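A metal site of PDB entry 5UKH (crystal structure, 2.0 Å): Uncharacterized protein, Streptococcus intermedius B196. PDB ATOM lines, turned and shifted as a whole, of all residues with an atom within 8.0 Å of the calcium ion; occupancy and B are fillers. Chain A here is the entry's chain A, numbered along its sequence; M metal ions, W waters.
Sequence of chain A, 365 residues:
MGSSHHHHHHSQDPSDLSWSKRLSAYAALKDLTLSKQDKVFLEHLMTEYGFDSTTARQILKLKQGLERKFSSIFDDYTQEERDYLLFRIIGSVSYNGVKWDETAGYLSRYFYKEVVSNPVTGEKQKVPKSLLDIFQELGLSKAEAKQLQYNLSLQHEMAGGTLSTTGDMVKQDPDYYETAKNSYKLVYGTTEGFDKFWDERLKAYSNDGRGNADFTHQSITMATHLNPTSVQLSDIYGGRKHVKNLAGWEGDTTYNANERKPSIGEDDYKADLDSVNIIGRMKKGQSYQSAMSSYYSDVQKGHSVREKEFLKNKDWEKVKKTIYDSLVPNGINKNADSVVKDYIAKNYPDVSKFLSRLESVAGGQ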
ATOM      1  N   TYR A  95       2.176  -2.589  18.680  1.00  0.00           N
ATOM      2  CA  TYR A  95       1.366  -3.753  19.005  1.00  0.00           C
ATOM      3  C   TYR A  95       0.644  -3.467  20.312  1.00  0.00           C
ATOM      4  O   TYR A  95       1.240  -3.491  21.391  1.00  0.00           O
ATOM      5  CB  TYR A  95       2.247  -5.012  19.082  1.00  0.00           C
ATOM      6  CG  TYR A  95       2.935  -5.311  17.766  1.00  0.00           C
ATOM      7  CD1 TYR A  95       2.283  -6.032  16.769  1.00  0.00           C
ATOM      8  CD2 TYR A  95       4.193  -4.834  17.498  1.00  0.00           C
ATOM      9  CE1 TYR A  95       2.896  -6.283  15.561  1.00  0.00           C
ATOM     10  CE2 TYR A  95       4.827  -5.096  16.296  1.00  0.00           C
ATOM     11  CZ  TYR A  95       4.174  -5.818  15.329  1.00  0.00           C
ATOM     12  OH  TYR A  95       4.822  -6.072  14.125  1.00  0.00           O
ATOM     13  N   GLN A 155      10.510   3.407  11.772  1.00  0.00           N
ATOM     14  CA  GLN A 155      11.373   2.250  11.523  1.00  0.00           C
ATOM     15  C   GLN A 155      10.525   1.017  11.259  1.00  0.00           C
ATOM     16  O   GLN A 155      10.797   0.247  10.329  1.00  0.00           O
ATOM     17  CB  GLN A 155      12.311   2.026  12.703  1.00  0.00           C
ATOM     18  CG  GLN A 155      13.608   1.257  12.339  1.00  0.00           C
ATOM     19  CD  GLN A 155      13.394  -0.252  12.295  1.00  0.00           C
ATOM     20  OE1 GLN A 155      12.375  -0.763  12.766  1.00  0.00           O
ATOM     21  NE2 GLN A 155      14.357  -0.959  11.723  1.00  0.00           N
ATOM     22  N   HIS A 156       9.432   0.869  12.016  1.00  0.00           N
ATOM     23  CA  HIS A 156       8.555  -0.277  11.869  1.00  0.00           C
ATOM     24  C   HIS A 156       7.906  -0.311  10.485  1.00  0.00           C
ATOM     25  O   HIS A 156       7.842  -1.372   9.857  1.00  0.00           O
ATOM     26  CB  HIS A 156       7.498  -0.234  12.964  1.00  0.00           C
ATOM     27  CG  HIS A 156       6.408  -1.243  12.794  1.00  0.00           C
ATOM     28  ND1 HIS A 156       6.603  -2.598  12.998  1.00  0.00           N
ATOM     29  CD2 HIS A 156       5.107  -1.098  12.456  1.00  0.00           C
ATOM     30  CE1 HIS A 156       5.460  -3.241  12.800  1.00  0.00           C
ATOM     31  NE2 HIS A 156       4.538  -2.360  12.461  1.00  0.00           N
ATOM     32  N   GLU A 157       7.425   0.837   9.995  1.00  0.00           N
ATOM     33  CA  GLU A 157       6.740   0.873   8.704  1.00  0.00           C
ATOM     34  C   GLU A 157       7.713   0.862   7.535  1.00  0.00           C
ATOM     35  O   GLU A 157       7.407   0.283   6.485  1.00  0.00           O
ATOM     36  CB  GLU A 157       5.844   2.117   8.606  1.00  0.00           C
ATOM     37  CG  GLU A 157       4.884   2.344   9.772  1.00  0.00           C
ATOM     38  CD  GLU A 157       4.304   3.779   9.724  1.00  0.00           C
ATOM     39  OE1 GLU A 157       3.663   4.118   8.702  1.00  0.00           O
ATOM     40  OE2 GLU A 157       4.518   4.557  10.677  1.00  0.00           O
ATOM     41  N   MET A 158       8.867   1.486   7.695  1.00  0.00           N
ATOM     42  CA  MET A 158       9.869   1.589   6.639  1.00  0.00           C
ATOM     43  C   MET A 158      10.848   0.379   6.540  1.00  0.00           C
ATOM     44  O   MET A 158      11.458   0.167   5.491  1.00  0.00           O
ATOM     45  CB  MET A 158      10.670   2.859   6.856  1.00  0.00           C
ATOM     46  CG  MET A 158       9.935   4.162   6.516  1.00  0.00           C
ATOM     47  SD  MET A 158      11.016   5.630   7.199  1.00  0.00           S
ATOM     48  CE  MET A 158      10.042   7.125   6.336  1.00  0.00           C
ATOM     49  N   ALA A 159      10.976  -0.430   7.607  1.00  0.00           N
ATOM     50  CA  ALA A 159      12.038  -1.446   7.654  1.00  0.00           C
ATOM     51  C   ALA A 159      11.969  -2.421   6.476  1.00  0.00           C
ATOM     52  O   ALA A 159      13.019  -2.884   5.998  1.00  0.00           O
ATOM     53  CB  ALA A 159      11.979  -2.228   8.966  1.00  0.00           C
ATOM     54  N   GLY A 160      10.770  -2.753   6.008  1.00  0.00           N
ATOM     55  CA  GLY A 160      10.608  -3.752   4.956  1.00  0.00           C
ATOM     56  C   GLY A 160      10.910  -3.298   3.535  1.00  0.00           C
ATOM     57  O   GLY A 160      10.900  -4.129   2.626  1.00  0.00           O
ATOM     58  N   ASN A 212      15.753  -3.948   6.696  1.00  0.00           N
ATOM     59  CA  ASN A 212      16.325  -4.118   8.021  1.00  0.00           C
ATOM     60  C   ASN A 212      15.315  -4.844   8.886  1.00  0.00           C
ATOM     61  O   ASN A 212      14.112  -4.781   8.631  1.00  0.00           O
ATOM     62  CB  ASN A 212      16.628  -2.777   8.694  1.00  0.00           C
ATOM     63  CG  ASN A 212      17.966  -2.214   8.309  1.00  0.00           C
ATOM     64  OD1 ASN A 212      18.859  -2.941   7.857  1.00  0.00           O
ATOM     65  ND2 ASN A 212      18.131  -0.904   8.481  1.00  0.00           N
ATOM     66  N   ALA A 213      15.808  -5.477   9.962  1.00  0.00           N
ATOM     67  CA  ALA A 213      14.902  -6.020  10.980  1.00  0.00           C
ATOM     68  C   ALA A 213      13.901  -4.975  11.477  1.00  0.00           C
ATOM     69  O   ALA A 213      14.270  -3.837  11.787  1.00  0.00           O
ATOM     70  CB  ALA A 213      15.717  -6.579  12.153  1.00  0.00           C
ATOM     71  N   ASP A 214      12.641  -5.383  11.558  1.00  0.00           N
ATOM     72  CA  ASP A 214      11.542  -4.570  12.101  1.00  0.00           C
ATOM     73  C   ASP A 214      11.653  -4.559  13.624  1.00  0.00           C
ATOM     74  O   ASP A 214      11.444  -5.580  14.275  1.00  0.00           O
ATOM     75  CB  ASP A 214      10.227  -5.168  11.616  1.00  0.00           C
ATOM     76  CG  ASP A 214       8.988  -4.464  12.123  1.00  0.00           C
ATOM     77  OD1 ASP A 214       9.003  -3.680  13.103  1.00  0.00           O
ATOM     78  OD2 ASP A 214       7.936  -4.776  11.521  1.00  0.00           O
ATOM     79  N   PHE A 215      12.069  -3.431  14.189  1.00  0.00           N
ATOM     80  CA  PHE A 215      12.509  -3.400  15.587  1.00  0.00           C
ATOM     81  C   PHE A 215      11.340  -3.587  16.566  1.00  0.00           C
ATOM     82  O   PHE A 215      11.467  -4.333  17.549  1.00  0.00           O
ATOM     83  CB  PHE A 215      13.259  -2.099  15.847  1.00  0.00           C
ATOM     84  CG  PHE A 215      13.828  -1.968  17.237  1.00  0.00           C
ATOM     85  CD1 PHE A 215      14.721  -2.926  17.749  1.00  0.00           C
ATOM     86  CD2 PHE A 215      13.513  -0.871  18.032  1.00  0.00           C
ATOM     87  CE1 PHE A 215      15.267  -2.784  19.035  1.00  0.00           C
ATOM     88  CE2 PHE A 215      14.068  -0.709  19.312  1.00  0.00           C
ATOM     89  CZ  PHE A 215      14.941  -1.672  19.814  1.00  0.00           C
ATOM     90  N   THR A 216      10.206  -2.905  16.334  1.00  0.00           N
ATOM     91  CA  THR A 216       9.081  -3.118  17.243  1.00  0.00           C
ATOM     92  C   THR A 216       8.516  -4.515  17.097  1.00  0.00           C
ATOM     93  O   THR A 216       8.026  -5.098  18.079  1.00  0.00           O
ATOM     94  CB  THR A 216       7.956  -2.061  17.073  1.00  0.00           C
ATOM     95  OG1 THR A 216       7.387  -2.125  15.750  1.00  0.00           O
ATOM     96  CG2 THR A 216       8.463  -0.698  17.355  1.00  0.00           C
ATOM     97  N   HIS A 217       8.583  -5.080  15.893  1.00  0.00           N
ATOM     98  CA  HIS A 217       8.124  -6.449  15.679  1.00  0.00           C
ATOM     99  C   HIS A 217       9.029  -7.429  16.437  1.00  0.00           C
ATOM    100  O   HIS A 217       8.547  -8.341  17.129  1.00  0.00           O
ATOM    101  CB  HIS A 217       8.100  -6.723  14.172  1.00  0.00           C
ATOM    102  CG  HIS A 217       7.667  -8.100  13.761  1.00  0.00           C
ATOM    103  ND1 HIS A 217       6.660  -8.320  12.851  1.00  0.00           N
ATOM    104  CD2 HIS A 217       8.158  -9.322  14.068  1.00  0.00           C
ATOM    105  CE1 HIS A 217       6.517  -9.608  12.647  1.00  0.00           C
ATOM    106  NE2 HIS A 217       7.416 -10.247  13.375  1.00  0.00           N
ATOM    107  N   GLN A 218      10.357  -7.254  16.310  1.00  0.00           N
ATOM    108  CA  GLN A 218      11.293  -8.074  17.064  1.00  0.00           C
ATOM    109  C   GLN A 218      11.042  -7.959  18.554  1.00  0.00           C
ATOM    110  O   GLN A 218      11.093  -8.954  19.296  1.00  0.00           O
ATOM    111  CB  GLN A 218      12.738  -7.683  16.748  1.00  0.00           C
ATOM    112  CG  GLN A 218      13.801  -8.638  17.332  1.00  0.00           C
ATOM    113  CD  GLN A 218      15.230  -8.249  16.915  1.00  0.00           C
ATOM    114  OE1 GLN A 218      15.428  -7.531  15.954  1.00  0.00           O
ATOM    115  NE2 GLN A 218      16.217  -8.758  17.645  1.00  0.00           N
ATOM    116  N   ASP A 252       4.012 -15.440  11.347  1.00  0.00           N
ATOM    117  CA  ASP A 252       4.233 -14.769  10.077  1.00  0.00           C
ATOM    118  C   ASP A 252       4.262 -15.706   8.887  1.00  0.00           C
ATOM    119  O   ASP A 252       4.152 -15.231   7.752  1.00  0.00           O
ATOM    120  CB  ASP A 252       5.549 -13.975  10.130  1.00  0.00           C
ATOM    121  CG  ASP A 252       5.497 -12.821  11.133  1.00  0.00           C
ATOM    122  OD1 ASP A 252       4.379 -12.422  11.548  1.00  0.00           O
ATOM    123  OD2 ASP A 252       6.567 -12.320  11.508  1.00  0.00           O
ATOM    124  N   SER A 263       2.711 -13.187   6.134  1.00  0.00           N
ATOM    125  CA  SER A 263       3.429 -12.027   5.638  1.00  0.00           C
ATOM    126  C   SER A 263       4.797 -12.052   6.297  1.00  0.00           C
ATOM    127  O   SER A 263       4.904 -11.835   7.513  1.00  0.00           O
ATOM    128  CB  SER A 263       2.687 -10.723   5.952  1.00  0.00           C
ATOM    129  OG  SER A 263       3.490  -9.597   5.658  1.00  0.00           O
ATOM    130  N   ILE A 264       5.843 -12.358   5.517  1.00  0.00           N
ATOM    131  CA  ILE A 264       7.187 -12.379   6.079  1.00  0.00           C
ATOM    132  C   ILE A 264       8.150 -11.695   5.120  1.00  0.00           C
ATOM    133  O   ILE A 264       9.049 -12.327   4.530  1.00  0.00           O
ATOM    134  CB  ILE A 264       7.614 -13.812   6.463  1.00  0.00           C
ATOM    135  CG1 ILE A 264       8.948 -13.809   7.213  1.00  0.00           C
ATOM    136  CG2 ILE A 264       7.629 -14.781   5.248  1.00  0.00           C
ATOM    137  CD1 ILE A 264       9.239 -15.125   7.885  1.00  0.00           C
ATOM    138  N   GLY A 265       7.977 -10.393   4.951  1.00  0.00           N
ATOM    139  CA  GLY A 265       8.959  -9.591   4.253  1.00  0.00           C
ATOM    140  C   GLY A 265      10.311  -9.649   4.947  1.00  0.00           C
ATOM    141  O   GLY A 265      10.483 -10.218   6.030  1.00  0.00           O
ATOM    142  N   GLU A 266      11.295  -9.019   4.294  1.00  0.00           N
ATOM    143  CA  GLU A 266      12.673  -9.117   4.769  1.00  0.00           C
ATOM    144  C   GLU A 266      12.819  -8.574   6.186  1.00  0.00           C
ATOM    145  O   GLU A 266      13.619  -9.086   6.984  1.00  0.00           O
ATOM    146  CB  GLU A 266      13.600  -8.350   3.824  1.00  0.00           C
ATOM    147  CG  GLU A 266      15.048  -8.416   4.226  1.00  0.00           C
ATOM    148  CD  GLU A 266      15.628  -9.803   4.030  1.00  0.00           C
ATOM    149  OE1 GLU A 266      15.146 -10.524   3.135  1.00  0.00           O
ATOM    150  OE2 GLU A 266      16.553 -10.169   4.779  1.00  0.00           O
ATOM    151  N   ASP A 267      12.072  -7.499   6.505  1.00  0.00           N
ATOM    152  CA  ASP A 267      12.102  -6.931   7.863  1.00  0.00           C
ATOM    153  C   ASP A 267      11.599  -7.919   8.904  1.00  0.00           C
ATOM    154  O   ASP A 267      12.080  -7.918  10.051  1.00  0.00           O
ATOM    155  CB  ASP A 267      11.271  -5.652   7.919  1.00  0.00           C
ATOM    156  CG  ASP A 267       9.800  -5.876   7.619  1.00  0.00           C
ATOM    157  OD1 ASP A 267       9.448  -6.664   6.718  1.00  0.00           O
ATOM    158  OD2 ASP A 267       8.977  -5.248   8.285  1.00  0.00           O
ATOM    159  N   ASP A 268      10.623  -8.752   8.559  1.00  0.00           N
ATOM    160  CA  ASP A 268      10.116  -9.687   9.553  1.00  0.00           C
ATOM    161  C   ASP A 268      10.894 -10.975   9.555  1.00  0.00           C
ATOM    162  O   ASP A 268      10.980 -11.631  10.591  1.00  0.00           O
ATOM    163  CB  ASP A 268       8.635  -9.941   9.294  1.00  0.00           C
ATOM    164  CG  ASP A 268       7.829  -8.664   9.448  1.00  0.00           C
ATOM    165  OD1 ASP A 268       8.170  -7.887  10.365  1.00  0.00           O
ATOM    166  OD2 ASP A 268       6.926  -8.400   8.612  1.00  0.00           O
ATOM    167  N   TYR A 269      11.472 -11.315   8.404  1.00  0.00           N
ATOM    168  CA  TYR A 269      12.422 -12.417   8.337  1.00  0.00           C
ATOM    169  C   TYR A 269      13.558 -12.206   9.344  1.00  0.00           C
ATOM    170  O   TYR A 269      13.820 -13.055  10.199  1.00  0.00           O
ATOM    171  CB  TYR A 269      12.958 -12.533   6.909  1.00  0.00           C
ATOM    172  CG  TYR A 269      14.015 -13.598   6.766  1.00  0.00           C
ATOM    173  CD1 TYR A 269      13.668 -14.922   6.568  1.00  0.00           C
ATOM    174  CD2 TYR A 269      15.358 -13.276   6.854  1.00  0.00           C
ATOM    175  CE1 TYR A 269      14.616 -15.900   6.459  1.00  0.00           C
ATOM    176  CE2 TYR A 269      16.323 -14.238   6.737  1.00  0.00           C
ATOM    177  CZ  TYR A 269      15.954 -15.551   6.531  1.00  0.00           C
ATOM    178  OH  TYR A 269      16.933 -16.513   6.418  1.00  0.00           O
ATOM    179  N   ALA A 271      13.727  -9.924  11.875  1.00  0.00           N
ATOM    180  CA  ALA A 271      13.183  -9.815  13.229  1.00  0.00           C
ATOM    181  C   ALA A 271      12.854 -11.192  13.816  1.00  0.00           C
ATOM    182  O   ALA A 271      13.178 -11.485  14.967  1.00  0.00           O
ATOM    183  CB  ALA A 271      11.938  -8.915  13.254  1.00  0.00           C
ATOM    184  N   ASP A 272      12.173 -12.024  13.043  1.00  0.00           N
ATOM    185  CA  ASP A 272      11.729 -13.306  13.578  1.00  0.00           C
ATOM    186  C   ASP A 272      12.914 -14.184  13.949  1.00  0.00           C
ATOM    187  O   ASP A 272      12.962 -14.767  15.034  1.00  0.00           O
ATOM    188  CB  ASP A 272      10.818 -14.003  12.584  1.00  0.00           C
ATOM    189  CG  ASP A 272       9.477 -13.324  12.461  1.00  0.00           C
ATOM    190  OD1 ASP A 272       9.169 -12.450  13.319  1.00  0.00           O
ATOM    191  OD2 ASP A 272       8.735 -13.673  11.516  1.00  0.00           O
HETATM  192 CA    CA M   1       6.965  -5.896   9.756  1.00  0.00          CA
HETATM  193  O   HOH W   1       6.053  -6.047   8.121  1.00  0.00           O
HETATM  194  O   HOH W   2       6.153  -3.493   9.484  1.00  0.00           O
HETATM  195  O   HOH W   3       4.582  -6.495  11.126  1.00  0.00           O
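ND1 of His 217 is in hydrogen-bond range of OH of Tyr 95 (3.2 Å). The side-chain carboxylate (OD2) of Asp 252 sits at hydrogen-bond distance from a ring nitrogen (NE2) of His 217 (2.9 Å). ND1 of His 217 lies close to OD1 of Asp 268 (2.9 Å). The side-chain carboxylate of Asp 272 sits at hydrogen-bond distance from a ring nitrogen (NE2) of His 217 (2.8 Å). The side-chain carboxylate (OD1) of Asp 214 sits at hydrogen-bond distance from the backbone NH (N) of His 217, 3.1 Å away. The side-chain carboxylate (OD1) of Asp 214 lies within hydrogen-bond range of a ring nitrogen (ND1) of His 156 (2.6 Å). The side-chain carboxylate (OD1) of Asp 214 lies within hydrogen-bond range of the side-chain hydroxyl (OG1) of Thr 216 (3.5 Å).
ND1 of His 217 touches the calcium ion, at 3.9 Å. Four residues have an atom within 4 Å of the calcium ion: Asp 214, His 217, Asp 267 and Asp 268. The nearest printed residue that does not touch the calcium ion is His 156 (4.3 Å).
The calcium ion is bound by water W1 (1.9 Å), the side-chain carboxylate (OD2) of Asp 214 (2.3 Å), the side-chain carboxylate (OD1) of Asp 268 (2.4 Å), water W2 (2.6 Å), the side-chain carboxylate (OD2) of Asp 267 (2.6 Å), the side-chain carboxylate (OD2) of Asp 268 (2.8 Å) and water W3 (2.8 Å). The calcium ion has seven donor atoms within binding distance.
Water W3 bridges the side-chain hydroxyl of Tyr 95 and a ring nitrogen (ND1) of His 217.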
